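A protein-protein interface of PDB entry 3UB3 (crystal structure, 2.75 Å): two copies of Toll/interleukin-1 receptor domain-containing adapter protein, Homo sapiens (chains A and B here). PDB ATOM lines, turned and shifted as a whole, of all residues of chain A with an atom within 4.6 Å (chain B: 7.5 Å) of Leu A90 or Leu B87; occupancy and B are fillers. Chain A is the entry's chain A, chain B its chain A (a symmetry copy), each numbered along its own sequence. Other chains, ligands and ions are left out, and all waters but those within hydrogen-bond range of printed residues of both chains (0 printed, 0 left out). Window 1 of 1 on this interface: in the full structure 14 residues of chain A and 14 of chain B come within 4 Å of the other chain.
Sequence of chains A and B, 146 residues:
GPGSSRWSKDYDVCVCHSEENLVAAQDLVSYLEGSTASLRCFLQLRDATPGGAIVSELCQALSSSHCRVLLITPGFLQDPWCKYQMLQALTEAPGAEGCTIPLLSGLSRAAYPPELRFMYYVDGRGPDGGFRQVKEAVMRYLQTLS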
ATOM      1  N   MET A  86     -11.825  -8.998 -28.025  1.00  0.00           N
ATOM      2  CA  MET A  86     -10.719  -9.662 -27.357  1.00  0.00           C
ATOM      3  C   MET A  86     -11.252 -10.926 -26.716  1.00  0.00           C
ATOM      4  O   MET A  86     -10.687 -12.003 -26.876  1.00  0.00           O
ATOM      5  CB  MET A  86     -10.124  -8.766 -26.280  1.00  0.00           C
ATOM      6  CG  MET A  86      -9.123  -9.470 -25.387  1.00  0.00           C
ATOM      7  SD  MET A  86      -8.145  -8.326 -24.387  1.00  0.00           S
ATOM      8  CE  MET A  86      -7.683  -9.381 -22.966  1.00  0.00           C
ATOM      9  N   LEU A  87     -12.346 -10.777 -25.981  1.00  0.00           N
ATOM     10  CA  LEU A  87     -12.997 -11.887 -25.300  1.00  0.00           C
ATOM     11  C   LEU A  87     -13.311 -13.017 -26.273  1.00  0.00           C
ATOM     12  O   LEU A  87     -12.875 -14.144 -26.079  1.00  0.00           O
ATOM     13  CB  LEU A  87     -14.287 -11.390 -24.658  1.00  0.00           C
ATOM     14  CG  LEU A  87     -15.068 -12.301 -23.718  1.00  0.00           C
ATOM     15  CD1 LEU A  87     -14.423 -12.290 -22.347  1.00  0.00           C
ATOM     16  CD2 LEU A  87     -16.505 -11.813 -23.632  1.00  0.00           C
ATOM     17  N   GLN A  88     -14.073 -12.715 -27.317  1.00  0.00           N
ATOM     18  CA  GLN A  88     -14.422 -13.730 -28.302  1.00  0.00           C
ATOM     19  C   GLN A  88     -13.196 -14.304 -29.002  1.00  0.00           C
ATOM     20  O   GLN A  88     -13.191 -15.458 -29.426  1.00  0.00           O
ATOM     21  CB  GLN A  88     -15.379 -13.158 -29.346  1.00  0.00           C
ATOM     22  CG  GLN A  88     -16.789 -12.930 -28.842  1.00  0.00           C
ATOM     23  CD  GLN A  88     -17.705 -12.426 -29.941  1.00  0.00           C
ATOM     24  OE1 GLN A  88     -17.454 -11.375 -30.540  1.00  0.00           O
ATOM     25  NE2 GLN A  88     -18.771 -13.171 -30.217  1.00  0.00           N
ATOM     26  N   ALA A  89     -12.159 -13.488 -29.130  1.00  0.00           N
ATOM     27  CA  ALA A  89     -10.926 -13.931 -29.759  1.00  0.00           C
ATOM     28  C   ALA A  89     -10.254 -14.992 -28.885  1.00  0.00           C
ATOM     29  O   ALA A  89      -9.481 -15.809 -29.373  1.00  0.00           O
ATOM     30  CB  ALA A  89     -10.000 -12.755 -29.950  1.00  0.00           C
ATOM     31  N   LEU A  90     -10.559 -14.971 -27.591  1.00  0.00           N
ATOM     32  CA  LEU A  90      -9.992 -15.921 -26.645  1.00  0.00           C
ATOM     33  C   LEU A  90     -11.009 -17.003 -26.278  1.00  0.00           C
ATOM     34  O   LEU A  90     -10.638 -18.067 -25.770  1.00  0.00           O
ATOM     35  CB  LEU A  90      -9.525 -15.186 -25.390  1.00  0.00           C
ATOM     36  CG  LEU A  90      -8.426 -14.144 -25.624  1.00  0.00           C
ATOM     37  CD1 LEU A  90      -8.233 -13.271 -24.398  1.00  0.00           C
ATOM     38  CD2 LEU A  90      -7.137 -14.857 -25.963  1.00  0.00           C
ATOM     39  N   THR A  91     -12.291 -16.729 -26.524  1.00  0.00           N
ATOM     40  CA  THR A  91     -13.340 -17.697 -26.218  1.00  0.00           C
ATOM     41  C   THR A  91     -13.103 -18.908 -27.102  1.00  0.00           C
ATOM     42  O   THR A  91     -12.652 -19.953 -26.629  1.00  0.00           O
ATOM     43  CB  THR A  91     -14.768 -17.148 -26.498  1.00  0.00           C
ATOM     44  OG1 THR A  91     -14.910 -16.845 -27.893  1.00  0.00           O
ATOM     45  CG2 THR A  91     -15.041 -15.903 -25.657  1.00  0.00           C
ATOM     46  N   GLU A  92     -13.402 -18.770 -28.391  1.00  0.00           N
ATOM     47  CA  GLU A  92     -13.170 -19.874 -29.306  1.00  0.00           C
ATOM     48  C   GLU A  92     -11.872 -19.628 -30.068  1.00  0.00           C
ATOM     49  O   GLU A  92     -11.862 -19.062 -31.162  1.00  0.00           O
ATOM     50  CB  GLU A  92     -14.345 -20.057 -30.267  1.00  0.00           C
ATOM     51  CG  GLU A  92     -14.501 -21.517 -30.705  1.00  0.00           C
ATOM     52  CD  GLU A  92     -14.262 -22.502 -29.552  1.00  0.00           C
ATOM     53  OE1 GLU A  92     -13.101 -22.621 -29.089  1.00  0.00           O
ATOM     54  OE2 GLU A  92     -15.232 -23.155 -29.102  1.00  0.00           O
ATOM     55  N   ALA A  93     -10.780 -20.065 -29.448  1.00  0.00           N
ATOM     56  CA  ALA A  93      -9.427 -19.913 -29.971  1.00  0.00           C
ATOM     57  C   ALA A  93      -8.520 -20.323 -28.796  1.00  0.00           C
ATOM     58  O   ALA A  93      -9.038 -20.783 -27.773  1.00  0.00           O
ATOM     59  CB  ALA A  93      -9.197 -18.462 -30.376  1.00  0.00           C
ATOM     60  N   THR A 100      -4.368 -17.171 -31.071  1.00  0.00           N
ATOM     61  CA  THR A 100      -4.622 -15.776 -30.731  1.00  0.00           C
ATOM     62  C   THR A 100      -3.394 -15.218 -30.021  1.00  0.00           C
ATOM     63  O   THR A 100      -3.014 -15.705 -28.959  1.00  0.00           O
ATOM     64  CB  THR A 100      -5.848 -15.637 -29.818  1.00  0.00           C
ATOM     65  OG1 THR A 100      -7.007 -16.081 -30.527  1.00  0.00           O
ATOM     66  CG2 THR A 100      -6.042 -14.188 -29.385  1.00  0.00           C
ATOM     67  N   MET A 119      -1.631 -16.623 -19.403  1.00  0.00           N
ATOM     68  CA  MET A 119      -1.795 -16.779 -20.840  1.00  0.00           C
ATOM     69  C   MET A 119      -0.569 -16.322 -21.604  1.00  0.00           C
ATOM     70  O   MET A 119       0.264 -15.584 -21.083  1.00  0.00           O
ATOM     71  CB  MET A 119      -2.992 -15.963 -21.315  1.00  0.00           C
ATOM     72  CG  MET A 119      -4.209 -16.108 -20.440  1.00  0.00           C
ATOM     73  SD  MET A 119      -5.550 -15.161 -21.112  1.00  0.00           S
ATOM     74  CE  MET A 119      -6.020 -16.291 -22.506  1.00  0.00           C
ATOM     75  N   LEU B  70     -20.713 -15.144 -11.707  1.00  0.00           N
ATOM     76  CA  LEU B  70     -19.429 -14.493 -11.441  1.00  0.00           C
ATOM     77  C   LEU B  70     -19.667 -13.313 -10.498  1.00  0.00           C
ATOM     78  O   LEU B  70     -20.240 -12.305 -10.896  1.00  0.00           O
ATOM     79  CB  LEU B  70     -18.819 -13.980 -12.745  1.00  0.00           C
ATOM     80  CG  LEU B  70     -18.695 -15.008 -13.870  1.00  0.00           C
ATOM     81  CD1 LEU B  70     -18.222 -14.303 -15.121  1.00  0.00           C
ATOM     82  CD2 LEU B  70     -17.723 -16.131 -13.488  1.00  0.00           C
ATOM     83  N   PHE B  76     -12.165  -9.234  -7.079  1.00  0.00           N
ATOM     84  CA  PHE B  76     -12.227 -10.160  -8.202  1.00  0.00           C
ATOM     85  C   PHE B  76     -11.460  -9.603  -9.408  1.00  0.00           C
ATOM     86  O   PHE B  76     -10.591 -10.273  -9.972  1.00  0.00           O
ATOM     87  CB  PHE B  76     -13.701 -10.403  -8.567  1.00  0.00           C
ATOM     88  CG  PHE B  76     -13.911 -11.413  -9.662  1.00  0.00           C
ATOM     89  CD1 PHE B  76     -13.643 -11.101 -10.992  1.00  0.00           C
ATOM     90  CD2 PHE B  76     -14.390 -12.685  -9.360  1.00  0.00           C
ATOM     91  CE1 PHE B  76     -13.849 -12.038 -12.005  1.00  0.00           C
ATOM     92  CE2 PHE B  76     -14.601 -13.631 -10.362  1.00  0.00           C
ATOM     93  CZ  PHE B  76     -14.331 -13.309 -11.689  1.00  0.00           C
ATOM     94  N   TRP B  81      -6.211 -14.710 -11.420  1.00  0.00           N
ATOM     95  CA  TRP B  81      -6.854 -16.019 -11.543  1.00  0.00           C
ATOM     96  C   TRP B  81      -8.369 -15.851 -11.697  1.00  0.00           C
ATOM     97  O   TRP B  81      -9.007 -16.589 -12.448  1.00  0.00           O
ATOM     98  CB  TRP B  81      -6.542 -16.889 -10.318  1.00  0.00           C
ATOM     99  CG  TRP B  81      -7.015 -18.305 -10.462  1.00  0.00           C
ATOM    100  CD1 TRP B  81      -7.846 -18.978  -9.619  1.00  0.00           C
ATOM    101  CD2 TRP B  81      -6.699 -19.219 -11.532  1.00  0.00           C
ATOM    102  NE1 TRP B  81      -8.073 -20.252 -10.092  1.00  0.00           N
ATOM    103  CE2 TRP B  81      -7.381 -20.429 -11.256  1.00  0.00           C
ATOM    104  CE3 TRP B  81      -5.904 -19.135 -12.685  1.00  0.00           C
ATOM    105  CZ2 TRP B  81      -7.300 -21.551 -12.104  1.00  0.00           C
ATOM    106  CZ3 TRP B  81      -5.823 -20.259 -13.535  1.00  0.00           C
ATOM    107  CH2 TRP B  81      -6.516 -21.449 -13.231  1.00  0.00           C
ATOM    108  N   CYS B  82      -8.932 -14.880 -10.980  1.00  0.00           N
ATOM    109  CA  CYS B  82     -10.359 -14.596 -11.067  1.00  0.00           C
ATOM    110  C   CYS B  82     -10.676 -14.196 -12.499  1.00  0.00           C
ATOM    111  O   CYS B  82     -11.598 -14.729 -13.115  1.00  0.00           O
ATOM    112  CB  CYS B  82     -10.753 -13.430 -10.156  1.00  0.00           C
ATOM    113  SG  CYS B  82     -10.571 -13.700  -8.378  1.00  0.00           S
ATOM    114  N   LYS B  83      -9.914 -13.237 -13.019  1.00  0.00           N
ATOM    115  CA  LYS B  83     -10.111 -12.745 -14.376  1.00  0.00           C
ATOM    116  C   LYS B  83      -9.976 -13.864 -15.384  1.00  0.00           C
ATOM    117  O   LYS B  83     -10.727 -13.939 -16.356  1.00  0.00           O
ATOM    118  CB  LYS B  83      -9.106 -11.636 -14.691  1.00  0.00           C
ATOM    119  CG  LYS B  83      -9.348 -10.340 -13.926  1.00  0.00           C
ATOM    120  CD  LYS B  83     -10.800  -9.866 -14.059  1.00  0.00           C
ATOM    121  CE  LYS B  83     -11.241  -9.772 -15.520  1.00  0.00           C
ATOM    122  NZ  LYS B  83     -10.391  -8.821 -16.294  1.00  0.00           N
ATOM    123  N   TYR B  84      -9.007 -14.738 -15.158  1.00  0.00           N
ATOM    124  CA  TYR B  84      -8.794 -15.852 -16.062  1.00  0.00           C
ATOM    125  C   TYR B  84     -10.024 -16.764 -16.038  1.00  0.00           C
ATOM    126  O   TYR B  84     -10.499 -17.196 -17.090  1.00  0.00           O
ATOM    127  CB  TYR B  84      -7.546 -16.632 -15.653  1.00  0.00           C
ATOM    128  CG  TYR B  84      -7.238 -17.771 -16.588  1.00  0.00           C
ATOM    129  CD1 TYR B  84      -6.773 -17.528 -17.877  1.00  0.00           C
ATOM    130  CD2 TYR B  84      -7.433 -19.096 -16.196  1.00  0.00           C
ATOM    131  CE1 TYR B  84      -6.508 -18.572 -18.758  1.00  0.00           C
ATOM    132  CE2 TYR B  84      -7.172 -20.155 -17.071  1.00  0.00           C
ATOM    133  CZ  TYR B  84      -6.709 -19.885 -18.352  1.00  0.00           C
ATOM    134  OH  TYR B  84      -6.450 -20.919 -19.224  1.00  0.00           O
ATOM    135  N   GLN B  85     -10.528 -17.053 -14.840  1.00  0.00           N
ATOM    136  CA  GLN B  85     -11.717 -17.887 -14.680  1.00  0.00           C
ATOM    137  C   GLN B  85     -12.917 -17.197 -15.328  1.00  0.00           C
ATOM    138  O   GLN B  85     -13.805 -17.853 -15.872  1.00  0.00           O
ATOM    139  CB  GLN B  85     -12.013 -18.154 -13.197  1.00  0.00           C
ATOM    140  CG  GLN B  85     -11.125 -19.236 -12.581  1.00  0.00           C
ATOM    141  CD  GLN B  85     -11.015 -20.485 -13.465  1.00  0.00           C
ATOM    142  OE1 GLN B  85     -12.024 -21.072 -13.868  1.00  0.00           O
ATOM    143  NE2 GLN B  85      -9.785 -20.893 -13.767  1.00  0.00           N
ATOM    144  N   MET B  86     -12.934 -15.869 -15.266  1.00  0.00           N
ATOM    145  CA  MET B  86     -14.004 -15.097 -15.873  1.00  0.00           C
ATOM    146  C   MET B  86     -13.964 -15.338 -17.367  1.00  0.00           C
ATOM    147  O   MET B  86     -14.980 -15.635 -17.987  1.00  0.00           O
ATOM    148  CB  MET B  86     -13.817 -13.611 -15.598  1.00  0.00           C
ATOM    149  CG  MET B  86     -14.758 -12.724 -16.389  1.00  0.00           C
ATOM    150  SD  MET B  86     -14.803 -11.024 -15.776  1.00  0.00           S
ATOM    151  CE  MET B  86     -15.310 -10.106 -17.274  1.00  0.00           C
ATOM    152  N   LEU B  87     -12.775 -15.197 -17.938  1.00  0.00           N
ATOM    153  CA  LEU B  87     -12.555 -15.399 -19.363  1.00  0.00           C
ATOM    154  C   LEU B  87     -13.060 -16.766 -19.806  1.00  0.00           C
ATOM    155  O   LEU B  87     -13.898 -16.862 -20.693  1.00  0.00           O
ATOM    156  CB  LEU B  87     -11.063 -15.283 -19.657  1.00  0.00           C
ATOM    157  CG  LEU B  87     -10.574 -15.260 -21.101  1.00  0.00           C
ATOM    158  CD1 LEU B  87     -10.760 -13.871 -21.678  1.00  0.00           C
ATOM    159  CD2 LEU B  87      -9.107 -15.656 -21.134  1.00  0.00           C
ATOM    160  N   GLN B  88     -12.545 -17.824 -19.190  1.00  0.00           N
ATOM    161  CA  GLN B  88     -12.972 -19.171 -19.545  1.00  0.00           C
ATOM    162  C   GLN B  88     -14.459 -19.393 -19.296  1.00  0.00           C
ATOM    163  O   GLN B  88     -15.103 -20.188 -19.977  1.00  0.00           O
ATOM    164  CB  GLN B  88     -12.169 -20.210 -18.766  1.00  0.00           C
ATOM    165  CG  GLN B  88     -10.735 -20.366 -19.229  1.00  0.00           C
ATOM    166  CD  GLN B  88     -10.011 -21.458 -18.463  1.00  0.00           C
ATOM    167  OE1 GLN B  88      -9.899 -21.399 -17.234  1.00  0.00           O
ATOM    168  NE2 GLN B  88      -9.520 -22.464 -19.180  1.00  0.00           N
ATOM    169  N   ALA B  89     -14.999 -18.692 -18.309  1.00  0.00           N
ATOM    170  CA  ALA B  89     -16.413 -18.802 -17.993  1.00  0.00           C
ATOM    171  C   ALA B  89     -17.243 -18.225 -19.140  1.00  0.00           C
ATOM    172  O   ALA B  89     -18.402 -18.583 -19.319  1.00  0.00           O
ATOM    173  CB  ALA B  89     -16.709 -18.060 -16.714  1.00  0.00           C
ATOM    174  N   LEU B  90     -16.638 -17.329 -19.915  1.00  0.00           N
ATOM    175  CA  LEU B  90     -17.310 -16.698 -21.042  1.00  0.00           C
ATOM    176  C   LEU B  90     -16.846 -17.306 -22.367  1.00  0.00           C
ATOM    177  O   LEU B  90     -17.518 -17.157 -23.394  1.00  0.00           O
ATOM    178  CB  LEU B  90     -17.042 -15.194 -21.027  1.00  0.00           C
ATOM    179  CG  LEU B  90     -17.557 -14.459 -19.785  1.00  0.00           C
ATOM    180  CD1 LEU B  90     -17.001 -13.049 -19.717  1.00  0.00           C
ATOM    181  CD2 LEU B  90     -19.068 -14.421 -19.829  1.00  0.00           C
ATOM    182  N   THR B  91     -15.696 -17.980 -22.348  1.00  0.00           N
ATOM    183  CA  THR B  91     -15.170 -18.605 -23.557  1.00  0.00           C
ATOM    184  C   THR B  91     -16.157 -19.682 -23.970  1.00  0.00           C
ATOM    185  O   THR B  91     -16.896 -19.516 -24.942  1.00  0.00           O
ATOM    186  CB  THR B  91     -13.778 -19.264 -23.340  1.00  0.00           C
ATOM    187  OG1 THR B  91     -13.881 -20.315 -22.368  1.00  0.00           O
ATOM    188  CG2 THR B  91     -12.755 -18.225 -22.885  1.00  0.00           C
ATOM    189  N   GLU B  92     -16.176 -20.786 -23.230  1.00  0.00           N
ATOM    190  CA  GLU B  92     -17.118 -21.847 -23.542  1.00  0.00           C
ATOM    191  C   GLU B  92     -18.305 -21.758 -22.590  1.00  0.00           C
ATOM    192  O   GLU B  92     -18.339 -22.395 -21.537  1.00  0.00           O
ATOM    193  CB  GLU B  92     -16.453 -23.223 -23.464  1.00  0.00           C
ATOM    194  CG  GLU B  92     -17.106 -24.224 -24.422  1.00  0.00           C
ATOM    195  CD  GLU B  92     -17.461 -23.593 -25.776  1.00  0.00           C
ATOM    196  OE1 GLU B  92     -18.381 -22.741 -25.824  1.00  0.00           O
ATOM    197  OE2 GLU B  92     -16.819 -23.943 -26.795  1.00  0.00           O
ATOM    198  N   ALA B  93     -19.272 -20.938 -22.993  1.00  0.00           N
ATOM    199  CA  ALA B  93     -20.488 -20.672 -22.233  1.00  0.00           C
ATOM    200  C   ALA B  93     -21.140 -19.487 -22.968  1.00  0.00           C
ATOM    201  O   ALA B  93     -20.646 -19.096 -24.031  1.00  0.00           O
ATOM    202  CB  ALA B  93     -20.123 -20.308 -20.799  1.00  0.00           C
ATOM    203  N   GLU B 115     -16.113  -4.804 -21.870  1.00  0.00           N
ATOM    204  CA  GLU B 115     -16.768  -5.837 -22.671  1.00  0.00           C
ATOM    205  C   GLU B 115     -18.223  -6.096 -22.284  1.00  0.00           C
ATOM    206  O   GLU B 115     -19.003  -6.638 -23.076  1.00  0.00           O
ATOM    207  CB  GLU B 115     -15.973  -7.150 -22.599  1.00  0.00           C
ATOM    208  CG  GLU B 115     -15.695  -7.640 -21.190  1.00  0.00           C
ATOM    209  CD  GLU B 115     -14.372  -7.140 -20.639  1.00  0.00           C
ATOM    210  OE1 GLU B 115     -13.876  -6.083 -21.088  1.00  0.00           O
ATOM    211  OE2 GLU B 115     -13.823  -7.804 -19.735  1.00  0.00           O
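Of the 10 printed residues of chain A, 5 touch a printed residue of chain B. Hydrophobic or aromatic side chains of chain A within 4 Å of the printed part of chain B: Leu A87, Leu A90 and Met A119. Hydrophobic or aromatic side chains of chain B that line the printed part of chain A: Tyr B84, Leu B87 and Leu B90. Among the printed residues, no Asp or Glu carboxylate lies within 4 Å of a Lys or Arg side-chain nitrogen of the other chain.
The side-chain carboxylate of Glu B92 sits close to the side-chain carboxylate of Glu A92 (2.9 Å).
Met A86 touches none of the printed residues of chain B. No residue of chain B comes within 4 Å of Ala A89. Leu A90 touches just these residues of chain B: Leu B87 and Thr B91. Printed residues of chain B within 4 Å of Thr A91: Leu B90 (3.6 Å) and Thr B91 (3.3 Å). Of the printed residues of chain A, Thr B91 touches Leu A90 (3.6 Å) and Thr A91 (3.3 Å). The nearest printed residue of chain A that does not touch Leu B90 is Glu A92 (6.7 Å).
The side-chain hydroxyl (OG1) of Thr A91 sits at hydrogen-bond distance from the backbone carbonyl oxygen (O) of Gln A88, at 2.7 Å. OH of Tyr B84 lies within hydrogen-bond range of NE2 of Gln B88 (3.4 Å). OG1 of Thr B91 lies within hydrogen-bond range of O of Gln B88 (2.7 Å).
Leu A87 touches Leu B90, and with the chains exchanged Leu A90 touches Leu B87. Leu A90 touches Thr B91, and with the chains exchanged Thr A91 touches Leu B90. Thr B91 touches its own counterpart, Thr A91. Glu B92 touches its own counterpart, Glu A92.
Among the printed residues, pairs that only touch across the chains: Thr A91 with Thr B91, Met A119 with Leu B87, Thr A91 with Leu B90, Leu A90 with Thr B91, Leu A87 with Leu B90, Leu A90 with Leu B87 and Met A119 with Tyr B84.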
